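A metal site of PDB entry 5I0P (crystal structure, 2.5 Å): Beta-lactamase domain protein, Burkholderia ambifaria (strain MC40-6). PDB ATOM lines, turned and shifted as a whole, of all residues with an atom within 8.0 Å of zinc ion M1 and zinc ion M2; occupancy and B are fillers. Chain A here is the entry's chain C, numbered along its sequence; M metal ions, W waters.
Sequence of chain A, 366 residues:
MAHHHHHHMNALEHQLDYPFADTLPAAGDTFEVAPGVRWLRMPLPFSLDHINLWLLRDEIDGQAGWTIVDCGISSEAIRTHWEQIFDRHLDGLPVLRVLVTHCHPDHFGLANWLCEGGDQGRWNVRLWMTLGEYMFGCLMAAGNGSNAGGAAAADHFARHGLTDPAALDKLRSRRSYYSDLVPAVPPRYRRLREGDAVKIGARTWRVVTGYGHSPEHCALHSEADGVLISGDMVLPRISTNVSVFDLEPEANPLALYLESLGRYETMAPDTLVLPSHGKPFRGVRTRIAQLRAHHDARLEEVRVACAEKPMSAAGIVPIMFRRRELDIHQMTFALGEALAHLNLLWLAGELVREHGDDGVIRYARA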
ATOM      1  N   LEU A  44      14.996 -18.910  23.666  1.00  0.00           N
ATOM      2  CA  LEU A  44      15.562 -19.882  22.760  1.00  0.00           C
ATOM      3  C   LEU A  44      14.898 -19.801  21.399  1.00  0.00           C
ATOM      4  O   LEU A  44      13.671 -19.706  21.311  1.00  0.00           O
ATOM      5  CB  LEU A  44      15.385 -21.298  23.297  1.00  0.00           C
ATOM      6  CG  LEU A  44      16.217 -21.622  24.497  1.00  0.00           C
ATOM      7  CD1 LEU A  44      15.777 -22.978  24.981  1.00  0.00           C
ATOM      8  CD2 LEU A  44      17.615 -21.648  23.965  1.00  0.00           C
ATOM      9  N   LEU A  48      10.704 -25.053  21.714  1.00  0.00           N
ATOM     10  CA  LEU A  48      10.873 -24.748  23.132  1.00  0.00           C
ATOM     11  C   LEU A  48      11.524 -23.371  23.213  1.00  0.00           C
ATOM     12  O   LEU A  48      12.685 -23.207  22.808  1.00  0.00           O
ATOM     13  CB  LEU A  48      11.694 -25.851  23.784  1.00  0.00           C
ATOM     14  CG  LEU A  48      11.792 -25.913  25.289  1.00  0.00           C
ATOM     15  CD1 LEU A  48      10.517 -26.485  25.801  1.00  0.00           C
ATOM     16  CD2 LEU A  48      12.922 -26.815  25.661  1.00  0.00           C
ATOM     17  N   HIS A  50      12.243 -21.073  25.552  1.00  0.00           N
ATOM     18  CA  HIS A  50      12.881 -20.460  26.692  1.00  0.00           C
ATOM     19  C   HIS A  50      13.568 -21.568  27.476  1.00  0.00           C
ATOM     20  O   HIS A  50      13.219 -22.740  27.331  1.00  0.00           O
ATOM     21  CB  HIS A  50      11.828 -19.782  27.563  1.00  0.00           C
ATOM     22  CG  HIS A  50      11.053 -20.768  28.363  1.00  0.00           C
ATOM     23  ND1 HIS A  50       9.915 -21.390  27.871  1.00  0.00           N
ATOM     24  CD2 HIS A  50      11.301 -21.327  29.578  1.00  0.00           C
ATOM     25  CE1 HIS A  50       9.470 -22.256  28.772  1.00  0.00           C
ATOM     26  NE2 HIS A  50      10.304 -22.238  29.807  1.00  0.00           N
ATOM     27  N   ILE A  51      14.548 -21.174  28.301  1.00  0.00           N
ATOM     28  CA  ILE A  51      15.119 -22.020  29.355  1.00  0.00           C
ATOM     29  C   ILE A  51      15.305 -21.161  30.608  1.00  0.00           C
ATOM     30  O   ILE A  51      15.704 -19.996  30.522  1.00  0.00           O
ATOM     31  CB  ILE A  51      16.461 -22.691  28.979  1.00  0.00           C
ATOM     32  CG1 ILE A  51      16.967 -23.550  30.175  1.00  0.00           C
ATOM     33  CG2 ILE A  51      17.528 -21.654  28.577  1.00  0.00           C
ATOM     34  CD1 ILE A  51      18.220 -24.359  29.880  1.00  0.00           C
ATOM     35  N   ASN A  52      15.012 -21.738  31.778  1.00  0.00           N
ATOM     36  CA  ASN A  52      15.213 -21.072  33.058  1.00  0.00           C
ATOM     37  C   ASN A  52      16.587 -21.468  33.600  1.00  0.00           C
ATOM     38  O   ASN A  52      16.926 -22.661  33.647  1.00  0.00           O
ATOM     39  CB  ASN A  52      14.137 -21.504  34.053  1.00  0.00           C
ATOM     40  CG  ASN A  52      12.745 -21.345  33.511  1.00  0.00           C
ATOM     41  OD1 ASN A  52      12.360 -20.293  32.968  1.00  0.00           O
ATOM     42  ND2 ASN A  52      11.957 -22.403  33.620  1.00  0.00           N
ATOM     43  N   ASP A  70      23.243 -23.786  35.064  1.00  0.00           N
ATOM     44  CA  ASP A  70      22.874 -23.823  33.630  1.00  0.00           C
ATOM     45  C   ASP A  70      23.046 -22.478  32.938  1.00  0.00           C
ATOM     46  O   ASP A  70      23.016 -21.419  33.596  1.00  0.00           O
ATOM     47  CB  ASP A  70      21.460 -24.334  33.420  1.00  0.00           C
ATOM     48  CG  ASP A  70      21.347 -25.841  33.638  1.00  0.00           C
ATOM     49  OD1 ASP A  70      20.219 -26.368  33.694  1.00  0.00           O
ATOM     50  OD2 ASP A  70      22.419 -26.470  33.746  1.00  0.00           O
ATOM     51  N   THR A 101      23.546 -28.954  34.838  1.00  0.00           N
ATOM     52  CA  THR A 101      22.724 -30.130  35.125  1.00  0.00           C
ATOM     53  C   THR A 101      22.977 -31.258  34.123  1.00  0.00           C
ATOM     54  O   THR A 101      22.921 -32.441  34.488  1.00  0.00           O
ATOM     55  CB  THR A 101      21.224 -29.774  35.154  1.00  0.00           C
ATOM     56  OG1 THR A 101      20.783 -29.271  33.853  1.00  0.00           O
ATOM     57  CG2 THR A 101      20.899 -28.759  36.268  1.00  0.00           C
ATOM     58  N   HIS A 102      23.201 -30.925  32.849  1.00  0.00           N
ATOM     59  CA  HIS A 102      23.422 -31.915  31.811  1.00  0.00           C
ATOM     60  C   HIS A 102      23.849 -31.180  30.545  1.00  0.00           C
ATOM     61  O   HIS A 102      23.772 -29.944  30.473  1.00  0.00           O
ATOM     62  CB  HIS A 102      22.199 -32.818  31.584  1.00  0.00           C
ATOM     63  CG  HIS A 102      21.017 -32.153  30.943  1.00  0.00           C
ATOM     64  ND1 HIS A 102      20.323 -31.120  31.551  1.00  0.00           N
ATOM     65  CD2 HIS A 102      20.345 -32.442  29.804  1.00  0.00           C
ATOM     66  CE1 HIS A 102      19.295 -30.778  30.793  1.00  0.00           C
ATOM     67  NE2 HIS A 102      19.288 -31.562  29.727  1.00  0.00           N
ATOM     68  N   CYS A 103      24.304 -31.950  29.555  1.00  0.00           N
ATOM     69  CA  CYS A 103      25.110 -31.436  28.444  1.00  0.00           C
ATOM     70  C   CYS A 103      24.301 -30.963  27.252  1.00  0.00           C
ATOM     71  O   CYS A 103      24.901 -30.529  26.260  1.00  0.00           O
ATOM     72  CB  CYS A 103      26.066 -32.518  27.965  1.00  0.00           C
ATOM     73  SG  CYS A 103      25.179 -33.888  27.139  1.00  0.00           S
ATOM     74  N   HIS A 104      22.974 -31.013  27.309  1.00  0.00           N
ATOM     75  CA  HIS A 104      22.197 -30.515  26.174  1.00  0.00           C
ATOM     76  C   HIS A 104      22.513 -29.029  25.930  1.00  0.00           C
ATOM     77  O   HIS A 104      22.793 -28.291  26.873  1.00  0.00           O
ATOM     78  CB  HIS A 104      20.704 -30.740  26.413  1.00  0.00           C
ATOM     79  CG  HIS A 104      20.303 -32.189  26.351  1.00  0.00           C
ATOM     80  ND1 HIS A 104      19.178 -32.693  26.950  1.00  0.00           N
ATOM     81  CD2 HIS A 104      20.931 -33.251  25.778  1.00  0.00           C
ATOM     82  CE1 HIS A 104      19.111 -33.999  26.742  1.00  0.00           C
ATOM     83  NE2 HIS A 104      20.159 -34.360  26.034  1.00  0.00           N
ATOM     84  N   PRO A 105      22.525 -28.590  24.668  1.00  0.00           N
ATOM     85  CA  PRO A 105      23.103 -27.276  24.337  1.00  0.00           C
ATOM     86  C   PRO A 105      22.472 -26.102  25.064  1.00  0.00           C
ATOM     87  O   PRO A 105      23.169 -25.120  25.310  1.00  0.00           O
ATOM     88  CB  PRO A 105      22.867 -27.163  22.823  1.00  0.00           C
ATOM     89  CG  PRO A 105      22.700 -28.511  22.375  1.00  0.00           C
ATOM     90  CD  PRO A 105      22.064 -29.290  23.467  1.00  0.00           C
ATOM     91  N   ASP A 106      21.181 -26.124  25.346  1.00  0.00           N
ATOM     92  CA  ASP A 106      20.590 -24.989  26.048  1.00  0.00           C
ATOM     93  C   ASP A 106      21.030 -24.912  27.508  1.00  0.00           C
ATOM     94  O   ASP A 106      20.944 -23.844  28.117  1.00  0.00           O
ATOM     95  CB  ASP A 106      19.061 -25.001  25.923  1.00  0.00           C
ATOM     96  CG  ASP A 106      18.465 -26.367  26.200  1.00  0.00           C
ATOM     97  OD1 ASP A 106      17.357 -26.364  26.774  1.00  0.00           O
ATOM     98  OD2 ASP A 106      19.065 -27.414  25.836  1.00  0.00           O
ATOM     99  N   HIS A 107      21.531 -26.011  28.091  1.00  0.00           N
ATOM    100  CA  HIS A 107      22.063 -25.947  29.441  1.00  0.00           C
ATOM    101  C   HIS A 107      23.566 -25.701  29.461  1.00  0.00           C
ATOM    102  O   HIS A 107      24.070 -25.075  30.390  1.00  0.00           O
ATOM    103  CB  HIS A 107      21.764 -27.235  30.196  1.00  0.00           C
ATOM    104  CG  HIS A 107      20.306 -27.536  30.256  1.00  0.00           C
ATOM    105  ND1 HIS A 107      19.564 -27.372  31.411  1.00  0.00           N
ATOM    106  CD2 HIS A 107      19.423 -27.855  29.288  1.00  0.00           C
ATOM    107  CE1 HIS A 107      18.301 -27.651  31.151  1.00  0.00           C
ATOM    108  NE2 HIS A 107      18.194 -27.948  29.875  1.00  0.00           N
ATOM    109  N   GLU A 133      27.825 -36.369  31.802  1.00  0.00           N
ATOM    110  CA  GLU A 133      27.412 -35.236  30.981  1.00  0.00           C
ATOM    111  C   GLU A 133      28.611 -34.537  30.365  1.00  0.00           C
ATOM    112  O   GLU A 133      28.634 -34.255  29.153  1.00  0.00           O
ATOM    113  CB  GLU A 133      26.574 -34.292  31.812  1.00  0.00           C
ATOM    114  CG  GLU A 133      25.401 -34.954  32.440  1.00  0.00           C
ATOM    115  CD  GLU A 133      24.317 -35.334  31.458  1.00  0.00           C
ATOM    116  OE1 GLU A 133      24.336 -34.803  30.331  1.00  0.00           O
ATOM    117  OE2 GLU A 133      23.416 -36.139  31.839  1.00  0.00           O
ATOM    118  N   HIS A 213      17.012 -39.421  30.014  1.00  0.00           N
ATOM    119  CA  HIS A 213      16.998 -38.201  29.212  1.00  0.00           C
ATOM    120  C   HIS A 213      18.385 -37.880  28.676  1.00  0.00           C
ATOM    121  O   HIS A 213      18.513 -37.334  27.581  1.00  0.00           O
ATOM    122  CB  HIS A 213      16.480 -37.040  30.069  1.00  0.00           C
ATOM    123  CG  HIS A 213      16.491 -35.723  29.370  1.00  0.00           C
ATOM    124  ND1 HIS A 213      15.591 -35.404  28.379  1.00  0.00           N
ATOM    125  CD2 HIS A 213      17.325 -34.666  29.480  1.00  0.00           C
ATOM    126  CE1 HIS A 213      15.873 -34.210  27.900  1.00  0.00           C
ATOM    127  NE2 HIS A 213      16.919 -33.738  28.549  1.00  0.00           N
ATOM    128  N   SER A 214      19.426 -38.179  29.448  1.00  0.00           N
ATOM    129  CA  SER A 214      20.801 -37.797  29.144  1.00  0.00           C
ATOM    130  C   SER A 214      21.707 -38.705  29.977  1.00  0.00           C
ATOM    131  O   SER A 214      21.216 -39.443  30.829  1.00  0.00           O
ATOM    132  CB  SER A 214      21.064 -36.314  29.474  1.00  0.00           C
ATOM    133  OG  SER A 214      20.842 -36.083  30.855  1.00  0.00           O
ATOM    134  N   HIS A 217      22.103 -37.139  34.408  1.00  0.00           N
ATOM    135  CA  HIS A 217      21.492 -35.840  34.666  1.00  0.00           C
ATOM    136  C   HIS A 217      21.573 -35.473  36.131  1.00  0.00           C
ATOM    137  O   HIS A 217      21.230 -36.292  36.988  1.00  0.00           O
ATOM    138  CB  HIS A 217      20.032 -35.867  34.272  1.00  0.00           C
ATOM    139  CG  HIS A 217      19.310 -34.568  34.460  1.00  0.00           C
ATOM    140  ND1 HIS A 217      18.916 -34.107  35.692  1.00  0.00           N
ATOM    141  CD2 HIS A 217      18.886 -33.645  33.560  1.00  0.00           C
ATOM    142  CE1 HIS A 217      18.266 -32.953  35.555  1.00  0.00           C
ATOM    143  NE2 HIS A 217      18.219 -32.663  34.266  1.00  0.00           N
ATOM    144  N   GLY A 231      16.132 -29.636  36.558  1.00  0.00           N
ATOM    145  CA  GLY A 231      16.670 -29.720  35.207  1.00  0.00           C
ATOM    146  C   GLY A 231      15.559 -30.057  34.232  1.00  0.00           C
ATOM    147  O   GLY A 231      14.446 -29.525  34.309  1.00  0.00           O
ATOM    148  N   ASP A 232      15.820 -31.026  33.352  1.00  0.00           N
ATOM    149  CA  ASP A 232      14.796 -31.481  32.419  1.00  0.00           C
ATOM    150  C   ASP A 232      14.073 -32.741  32.866  1.00  0.00           C
ATOM    151  O   ASP A 232      13.263 -33.267  32.088  1.00  0.00           O
ATOM    152  CB  ASP A 232      15.393 -31.754  31.042  1.00  0.00           C
ATOM    153  CG  ASP A 232      15.674 -30.499  30.272  1.00  0.00           C
ATOM    154  OD1 ASP A 232      15.313 -29.386  30.701  1.00  0.00           O
ATOM    155  OD2 ASP A 232      16.269 -30.660  29.207  1.00  0.00           O
ATOM    156  N   MET A 233      14.327 -33.243  34.069  1.00  0.00           N
ATOM    157  CA  MET A 233      13.740 -34.522  34.436  1.00  0.00           C
ATOM    158  C   MET A 233      12.271 -34.397  34.804  1.00  0.00           C
ATOM    159  O   MET A 233      11.495 -35.334  34.607  1.00  0.00           O
ATOM    160  CB  MET A 233      14.567 -35.153  35.576  1.00  0.00           C
ATOM    161  CG  MET A 233      15.964 -35.592  35.109  1.00  0.00           C
ATOM    162  SD  MET A 233      15.907 -37.072  34.056  1.00  0.00           S
ATOM    163  CE  MET A 233      15.281 -38.257  35.217  1.00  0.00           C
ATOM    164  N   LEU A 235       9.380 -31.564  34.104  1.00  0.00           N
ATOM    165  CA  LEU A 235       8.902 -30.325  33.543  1.00  0.00           C
ATOM    166  C   LEU A 235       7.392 -30.220  33.685  1.00  0.00           C
ATOM    167  O   LEU A 235       6.673 -31.198  33.469  1.00  0.00           O
ATOM    168  CB  LEU A 235       9.279 -30.226  32.066  1.00  0.00           C
ATOM    169  CG  LEU A 235      10.773 -30.417  31.938  1.00  0.00           C
ATOM    170  CD1 LEU A 235      11.079 -30.703  30.419  1.00  0.00           C
ATOM    171  CD2 LEU A 235      11.523 -29.171  32.477  1.00  0.00           C
ATOM    172  N   ILE A 238       5.577 -29.880  29.626  1.00  0.00           N
ATOM    173  CA  ILE A 238       5.923 -30.819  28.567  1.00  0.00           C
ATOM    174  C   ILE A 238       6.474 -32.091  29.190  1.00  0.00           C
ATOM    175  O   ILE A 238       6.954 -32.119  30.322  1.00  0.00           O
ATOM    176  CB  ILE A 238       6.941 -30.248  27.557  1.00  0.00           C
ATOM    177  CG1 ILE A 238       8.246 -29.982  28.290  1.00  0.00           C
ATOM    178  CG2 ILE A 238       6.460 -28.945  26.975  1.00  0.00           C
ATOM    179  CD1 ILE A 238       9.297 -29.319  27.483  1.00  0.00           C
ATOM    180  N   THR A 240       9.335 -35.049  29.212  1.00  0.00           N
ATOM    181  CA  THR A 240      10.797 -35.045  29.051  1.00  0.00           C
ATOM    182  C   THR A 240      11.182 -35.934  27.880  1.00  0.00           C
ATOM    183  O   THR A 240      10.774 -37.100  27.835  1.00  0.00           O
ATOM    184  CB  THR A 240      11.481 -35.598  30.308  1.00  0.00           C
ATOM    185  OG1 THR A 240      11.148 -34.789  31.441  1.00  0.00           O
ATOM    186  CG2 THR A 240      13.002 -35.637  30.105  1.00  0.00           C
ATOM    187  N   ASN A 241      12.035 -35.422  26.989  1.00  0.00           N
ATOM    188  CA  ASN A 241      12.458 -36.209  25.836  1.00  0.00           C
ATOM    189  C   ASN A 241      13.227 -37.463  26.267  1.00  0.00           C
ATOM    190  O   ASN A 241      14.147 -37.417  27.101  1.00  0.00           O
ATOM    191  CB  ASN A 241      13.301 -35.382  24.873  1.00  0.00           C
ATOM    192  CG  ASN A 241      13.883 -36.222  23.722  1.00  0.00           C
ATOM    193  OD1 ASN A 241      15.094 -36.451  23.648  1.00  0.00           O
ATOM    194  ND2 ASN A 241      13.008 -36.738  22.854  1.00  0.00           N
ATOM    195  N   PRO A 275      11.943 -26.042  37.404  1.00  0.00           N
ATOM    196  CA  PRO A 275      12.256 -26.793  36.191  1.00  0.00           C
ATOM    197  C   PRO A 275      12.949 -25.920  35.146  1.00  0.00           C
ATOM    198  O   PRO A 275      12.841 -24.694  35.122  1.00  0.00           O
ATOM    199  CB  PRO A 275      10.861 -27.176  35.692  1.00  0.00           C
ATOM    200  CG  PRO A 275      10.054 -25.831  36.033  1.00  0.00           C
ATOM    201  CD  PRO A 275      10.632 -25.373  37.341  1.00  0.00           C
ATOM    202  N   SER A 276      13.677 -26.577  34.258  1.00  0.00           N
ATOM    203  CA  SER A 276      14.427 -25.801  33.282  1.00  0.00           C
ATOM    204  C   SER A 276      13.550 -25.189  32.191  1.00  0.00           C
ATOM    205  O   SER A 276      14.013 -24.281  31.516  1.00  0.00           O
ATOM    206  CB  SER A 276      15.508 -26.678  32.661  1.00  0.00           C
ATOM    207  OG  SER A 276      16.520 -26.922  33.605  1.00  0.00           O
ATOM    208  N   HIS A 277      12.297 -25.642  32.033  1.00  0.00           N
ATOM    209  CA  HIS A 277      11.353 -25.103  31.073  1.00  0.00           C
ATOM    210  C   HIS A 277       9.986 -25.144  31.740  1.00  0.00           C
ATOM    211  O   HIS A 277       9.652 -26.163  32.359  1.00  0.00           O
ATOM    212  CB  HIS A 277      11.340 -25.907  29.734  1.00  0.00           C
ATOM    213  CG  HIS A 277      12.713 -26.204  29.227  1.00  0.00           C
ATOM    214  ND1 HIS A 277      13.401 -25.360  28.396  1.00  0.00           N
ATOM    215  CD2 HIS A 277      13.580 -27.192  29.561  1.00  0.00           C
ATOM    216  CE1 HIS A 277      14.617 -25.848  28.163  1.00  0.00           C
ATOM    217  NE2 HIS A 277      14.755 -26.947  28.886  1.00  0.00           N
HETATM  218 ZN    ZN M   1      16.455 -28.387  28.424  1.00  0.00          ZN
HETATM  219 ZN    ZN M   2      17.747 -31.640  28.085  1.00  0.00          ZN
HETATM  220  O   HOH W   1      15.431 -30.413  26.154  1.00  0.00           O
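A ring nitrogen (ND1) of His 107 sits at hydrogen-bond distance from the side-chain hydroxyl (OG1) of Thr 101 (3.3 Å). NE2 of His 277 lies close to OD1 of Asp 106 (3.4 Å). The backbone NH (N) of Asp 232 lies within hydrogen-bond range of a ring nitrogen (NE2) of His 217, at 3.0 Å. OD1 of Asp 70 lies within hydrogen-bond range of ND1 of His 107 (2.6 Å). ND1 of His 213 sits at hydrogen-bond distance from O of Asn 241, at 2.8 Å. The side-chain hydroxyl (OG1) of Thr 240 lies within hydrogen-bond range of the backbone carbonyl oxygen (O) of Asp 232, at 2.7 Å. The side-chain hydroxyl (OG1) of Thr 101 sits at hydrogen-bond distance from a ring nitrogen (ND1) of His 102 (3.0 Å). A ring nitrogen (ND1) of His 277 sits at hydrogen-bond distance from the backbone carbonyl oxygen (O) of His 50, 2.8 Å away.
Of the 27 residues printed, 4 come within 4 Å of zinc ion M2. The nearest printed residue that does not touch zinc ion M2 is His 107 (4.1 Å).
Zinc ion M1 is bound by NE2 of His 277 (2.3 Å), NE2 of His 107 (2.3 Å) and OD2 of Asp 232 (2.4 Å). Slightly farther from zinc ion M1 lies OD1 of Asp 232 (2.7 Å). Slightly farther from zinc ion M1 lies OD1 of Asp 106 (2.8 Å).
Zinc ion M2 is bound by the side-chain carboxylate (OD2) of Asp 232, a ring nitrogen (ND1) of His 104, a ring nitrogen (NE2) of His 102 and a ring nitrogen (NE2) of His 213. Zinc ion M2 has four donor atoms within binding distance.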
